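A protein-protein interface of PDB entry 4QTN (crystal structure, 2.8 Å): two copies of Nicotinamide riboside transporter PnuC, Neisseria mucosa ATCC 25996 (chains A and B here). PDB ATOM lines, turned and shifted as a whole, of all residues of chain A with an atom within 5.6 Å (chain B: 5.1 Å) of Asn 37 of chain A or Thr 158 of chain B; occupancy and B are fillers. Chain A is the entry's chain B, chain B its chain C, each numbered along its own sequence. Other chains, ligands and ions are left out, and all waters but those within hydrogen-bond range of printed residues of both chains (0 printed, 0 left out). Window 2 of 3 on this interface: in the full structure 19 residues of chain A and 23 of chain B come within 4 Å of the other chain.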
ATOM      1  N   VAL A  33      26.551  22.429  10.348  1.00  0.00           N
ATOM      2  CA  VAL A  33      25.310  22.231   9.600  1.00  0.00           C
ATOM      3  C   VAL A  33      25.303  23.038   8.314  1.00  0.00           C
ATOM      4  O   VAL A  33      24.811  22.577   7.296  1.00  0.00           O
ATOM      5  CB  VAL A  33      24.074  22.568  10.479  1.00  0.00           C
ATOM      6  CG1 VAL A  33      23.246  23.719   9.898  1.00  0.00           C
ATOM      7  CG2 VAL A  33      23.242  21.317  10.721  1.00  0.00           C
ATOM      8  N   PHE A  34      25.895  24.233   8.373  1.00  0.00           N
ATOM      9  CA  PHE A  34      25.936  25.177   7.255  1.00  0.00           C
ATOM     10  C   PHE A  34      27.051  24.825   6.270  1.00  0.00           C
ATOM     11  O   PHE A  34      26.923  25.034   5.063  1.00  0.00           O
ATOM     12  CB  PHE A  34      26.148  26.589   7.805  1.00  0.00           C
ATOM     13  CG  PHE A  34      26.497  27.603   6.764  1.00  0.00           C
ATOM     14  CD1 PHE A  34      27.806  27.724   6.302  1.00  0.00           C
ATOM     15  CD2 PHE A  34      25.527  28.462   6.264  1.00  0.00           C
ATOM     16  CE1 PHE A  34      28.125  28.657   5.345  1.00  0.00           C
ATOM     17  CE2 PHE A  34      25.844  29.402   5.311  1.00  0.00           C
ATOM     18  CZ  PHE A  34      27.144  29.500   4.849  1.00  0.00           C
ATOM     19  N   VAL A  35      28.148  24.307   6.796  1.00  0.00           N
ATOM     20  CA  VAL A  35      29.227  23.806   5.968  1.00  0.00           C
ATOM     21  C   VAL A  35      28.764  22.538   5.209  1.00  0.00           C
ATOM     22  O   VAL A  35      29.527  21.913   4.468  1.00  0.00           O
ATOM     23  CB  VAL A  35      30.504  23.557   6.821  1.00  0.00           C
ATOM     24  CG1 VAL A  35      31.534  22.743   6.058  1.00  0.00           C
ATOM     25  CG2 VAL A  35      31.106  24.888   7.258  1.00  0.00           C
ATOM     26  N   PHE A  36      27.495  22.190   5.379  1.00  0.00           N
ATOM     27  CA  PHE A  36      26.903  21.080   4.643  1.00  0.00           C
ATOM     28  C   PHE A  36      25.877  21.590   3.646  1.00  0.00           C
ATOM     29  O   PHE A  36      25.831  21.140   2.505  1.00  0.00           O
ATOM     30  CB  PHE A  36      26.267  20.060   5.605  1.00  0.00           C
ATOM     31  CG  PHE A  36      27.143  18.866   5.895  1.00  0.00           C
ATOM     32  CD1 PHE A  36      27.188  17.780   5.011  1.00  0.00           C
ATOM     33  CD2 PHE A  36      27.913  18.808   7.060  1.00  0.00           C
ATOM     34  CE1 PHE A  36      27.988  16.667   5.279  1.00  0.00           C
ATOM     35  CE2 PHE A  36      28.715  17.694   7.330  1.00  0.00           C
ATOM     36  CZ  PHE A  36      28.753  16.623   6.435  1.00  0.00           C
ATOM     37  N   ASN A  37      25.061  22.540   4.087  1.00  0.00           N
ATOM     38  CA  ASN A  37      24.044  23.137   3.250  1.00  0.00           C
ATOM     39  C   ASN A  37      24.203  24.632   3.220  1.00  0.00           C
ATOM     40  O   ASN A  37      23.438  25.343   3.878  1.00  0.00           O
ATOM     41  CB  ASN A  37      22.647  22.795   3.778  1.00  0.00           C
ATOM     42  CG  ASN A  37      22.317  21.325   3.652  1.00  0.00           C
ATOM     43  OD1 ASN A  37      21.183  20.954   3.328  1.00  0.00           O
ATOM     44  ND2 ASN A  37      23.307  20.472   3.906  1.00  0.00           N
ATOM     45  N   PRO A  38      25.208  25.140   2.465  1.00  0.00           N
ATOM     46  CA  PRO A  38      25.304  26.595   2.359  1.00  0.00           C
ATOM     47  C   PRO A  38      24.006  27.146   1.774  1.00  0.00           C
ATOM     48  O   PRO A  38      23.688  28.330   1.947  1.00  0.00           O
ATOM     49  CB  PRO A  38      26.476  26.799   1.382  1.00  0.00           C
ATOM     50  CG  PRO A  38      27.254  25.526   1.435  1.00  0.00           C
ATOM     51  CD  PRO A  38      26.226  24.461   1.639  1.00  0.00           C
ATOM     52  N   ASP A  39      23.221  26.238   1.194  1.00  0.00           N
ATOM     53  CA  ASP A  39      22.091  26.561   0.335  1.00  0.00           C
ATOM     54  C   ASP A  39      21.062  27.485   0.979  1.00  0.00           C
ATOM     55  O   ASP A  39      20.661  28.475   0.381  1.00  0.00           O
ATOM     56  CB  ASP A  39      21.440  25.273  -0.159  1.00  0.00           C
ATOM     57  CG  ASP A  39      22.467  24.204  -0.509  1.00  0.00           C
ATOM     58  OD1 ASP A  39      23.365  23.940   0.327  1.00  0.00           O
ATOM     59  OD2 ASP A  39      22.388  23.646  -1.626  1.00  0.00           O
ATOM     60  N   SER A  40      20.644  27.170   2.197  1.00  0.00           N
ATOM     61  CA  SER A  40      19.835  28.110   2.962  1.00  0.00           C
ATOM     62  C   SER A  40      20.576  28.618   4.184  1.00  0.00           C
ATOM     63  O   SER A  40      20.319  28.179   5.311  1.00  0.00           O
ATOM     64  CB  SER A  40      18.493  27.508   3.356  1.00  0.00           C
ATOM     65  OG  SER A  40      17.626  28.521   3.829  1.00  0.00           O
ATOM     66  N   TRP A  41      21.525  29.520   3.937  1.00  0.00           N
ATOM     67  CA  TRP A  41      22.172  30.289   4.983  1.00  0.00           C
ATOM     68  C   TRP A  41      21.099  30.969   5.838  1.00  0.00           C
ATOM     69  O   TRP A  41      21.195  31.012   7.065  1.00  0.00           O
ATOM     70  CB  TRP A  41      23.085  31.350   4.354  1.00  0.00           C
ATOM     71  CG  TRP A  41      22.335  32.304   3.480  1.00  0.00           C
ATOM     72  CD1 TRP A  41      21.765  32.025   2.281  1.00  0.00           C
ATOM     73  CD2 TRP A  41      22.006  33.679   3.773  1.00  0.00           C
ATOM     74  NE1 TRP A  41      21.126  33.140   1.785  1.00  0.00           N
ATOM     75  CE2 TRP A  41      21.255  34.167   2.682  1.00  0.00           C
ATOM     76  CE3 TRP A  41      22.285  34.542   4.845  1.00  0.00           C
ATOM     77  CZ2 TRP A  41      20.777  35.492   2.624  1.00  0.00           C
ATOM     78  CZ3 TRP A  41      21.804  35.855   4.793  1.00  0.00           C
ATOM     79  CH2 TRP A  41      21.062  36.315   3.684  1.00  0.00           C
ATOM     80  N   SER A  44      20.237  29.182   8.755  1.00  0.00           N
ATOM     81  CA  SER A  44      21.445  29.011   9.582  1.00  0.00           C
ATOM     82  C   SER A  44      21.751  30.265  10.354  1.00  0.00           C
ATOM     83  O   SER A  44      22.230  30.218  11.469  1.00  0.00           O
ATOM     84  CB  SER A  44      22.655  28.620   8.731  1.00  0.00           C
ATOM     85  OG  SER A  44      22.632  27.240   8.404  1.00  0.00           O
ATOM     86  N   LEU A 208      16.666  21.900   8.717  1.00  0.00           N
ATOM     87  CA  LEU A 208      17.536  21.367   9.741  1.00  0.00           C
ATOM     88  C   LEU A 208      18.047  22.397  10.763  1.00  0.00           C
ATOM     89  O   LEU A 208      17.986  22.146  11.947  1.00  0.00           O
ATOM     90  CB  LEU A 208      18.697  20.610   9.136  1.00  0.00           C
ATOM     91  CG  LEU A 208      19.125  19.492  10.063  1.00  0.00           C
ATOM     92  CD1 LEU A 208      18.292  18.252   9.771  1.00  0.00           C
ATOM     93  CD2 LEU A 208      20.603  19.201   9.918  1.00  0.00           C
ATOM     94  N   LEU B 156      25.633  10.827   1.309  1.00  0.00           N
ATOM     95  CA  LEU B 156      25.388  11.072   2.713  1.00  0.00           C
ATOM     96  C   LEU B 156      24.399  12.204   2.840  1.00  0.00           C
ATOM     97  O   LEU B 156      24.689  13.327   2.426  1.00  0.00           O
ATOM     98  CB  LEU B 156      26.690  11.444   3.423  1.00  0.00           C
ATOM     99  CG  LEU B 156      26.961  10.734   4.743  1.00  0.00           C
ATOM    100  CD1 LEU B 156      26.611   9.264   4.586  1.00  0.00           C
ATOM    101  CD2 LEU B 156      28.418  10.900   5.138  1.00  0.00           C
ATOM    102  N   PRO B 157      23.201  11.924   3.395  1.00  0.00           N
ATOM    103  CA  PRO B 157      22.357  13.066   3.637  1.00  0.00           C
ATOM    104  C   PRO B 157      23.017  13.930   4.692  1.00  0.00           C
ATOM    105  O   PRO B 157      23.832  13.439   5.469  1.00  0.00           O
ATOM    106  CB  PRO B 157      21.054  12.440   4.171  1.00  0.00           C
ATOM    107  CG  PRO B 157      21.133  10.989   3.798  1.00  0.00           C
ATOM    108  CD  PRO B 157      22.586  10.679   3.886  1.00  0.00           C
ATOM    109  N   THR B 158      22.709  15.214   4.669  1.00  0.00           N
ATOM    110  CA  THR B 158      23.417  16.186   5.466  1.00  0.00           C
ATOM    111  C   THR B 158      23.437  15.767   6.931  1.00  0.00           C
ATOM    112  O   THR B 158      24.487  15.717   7.558  1.00  0.00           O
ATOM    113  CB  THR B 158      22.777  17.573   5.314  1.00  0.00           C
ATOM    114  OG1 THR B 158      21.718  17.719   6.261  1.00  0.00           O
ATOM    115  CG2 THR B 158      22.197  17.748   3.871  1.00  0.00           C
ATOM    116  N   LEU B 159      22.276  15.426   7.465  1.00  0.00           N
ATOM    117  CA  LEU B 159      22.197  15.075   8.869  1.00  0.00           C
ATOM    118  C   LEU B 159      22.984  13.816   9.175  1.00  0.00           C
ATOM    119  O   LEU B 159      23.726  13.792  10.133  1.00  0.00           O
ATOM    120  CB  LEU B 159      20.754  14.950   9.345  1.00  0.00           C
ATOM    121  CG  LEU B 159      20.608  14.393  10.764  1.00  0.00           C
ATOM    122  CD1 LEU B 159      19.293  14.821  11.385  1.00  0.00           C
ATOM    123  CD2 LEU B 159      20.726  12.872  10.763  1.00  0.00           C
ATOM    124  N   ASP B 160      22.828  12.772   8.354  1.00  0.00           N
ATOM    125  CA  ASP B 160      23.633  11.556   8.522  1.00  0.00           C
ATOM    126  C   ASP B 160      25.078  11.980   8.514  1.00  0.00           C
ATOM    127  O   ASP B 160      25.946  11.313   9.092  1.00  0.00           O
ATOM    128  CB  ASP B 160      23.405  10.553   7.376  1.00  0.00           C
ATOM    129  CG  ASP B 160      21.921  10.202   7.162  1.00  0.00           C
ATOM    130  OD1 ASP B 160      21.062  11.114   7.216  1.00  0.00           O
ATOM    131  OD2 ASP B 160      21.626   9.016   6.881  1.00  0.00           O
ATOM    132  N   GLY B 161      25.334  13.110   7.856  1.00  0.00           N
ATOM    133  CA  GLY B 161      26.683  13.651   7.738  1.00  0.00           C
ATOM    134  C   GLY B 161      27.151  14.343   9.005  1.00  0.00           C
ATOM    135  O   GLY B 161      28.237  14.048   9.506  1.00  0.00           O
ATOM    136  N   VAL B 162      26.318  15.263   9.519  1.00  0.00           N
ATOM    137  CA  VAL B 162      26.612  16.037  10.750  1.00  0.00           C
ATOM    138  C   VAL B 162      26.957  15.135  11.928  1.00  0.00           C
ATOM    139  O   VAL B 162      27.974  15.336  12.593  1.00  0.00           O
ATOM    140  CB  VAL B 162      25.434  16.983  11.150  1.00  0.00           C
ATOM    141  CG1 VAL B 162      25.586  17.469  12.578  1.00  0.00           C
ATOM    142  CG2 VAL B 162      25.354  18.171  10.207  1.00  0.00           C
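Among the printed residues, merely in contact across the chains: Val 33 of chain A with Val 162 of chain B (3.8 Å), Phe 36 of chain A with Gly 161 of chain B (3.8 Å), Asn 37 of chain A with Thr 158 of chain B (2.9 Å) and Leu 208 of chain A with Leu 159 of chain B (3.9 Å).
Printed residues of chain A that touch a printed residue of chain B: Val 33, Phe 36, Asn 37 and Leu 208.
Hydrophobic or aromatic side chains of chain B within 4 Å of the printed part of chain A: Leu 159 and Val 162.
Among the printed residues, no Asp or Glu carboxylate lies within 4 Å of a Lys or Arg side-chain nitrogen of the other chain.
Of the printed residues of chain B, Phe 36 of chain A touches Gly 161 (3.8 Å).
Of the printed residues of chain B, Asn 37 of chain A touches Thr 158.
Printed residues of chain A within 4 Å of Thr 158 of chain B: Asn 37.
Printed residues of chain A within 4 Å of Gly 161 of chain B: Phe 36.
Printed residues of chain A within 4 Å of Val 162 of chain B: Val 33.
The nearest printed residue of chain B that does not touch Asn 37 of chain A is Leu 159 of chain B (6.3 Å).
The nearest printed residue of chain A that does not touch Thr 158 of chain B is Leu 208 of chain A (4.1 Å).
No position is printed for both chains.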
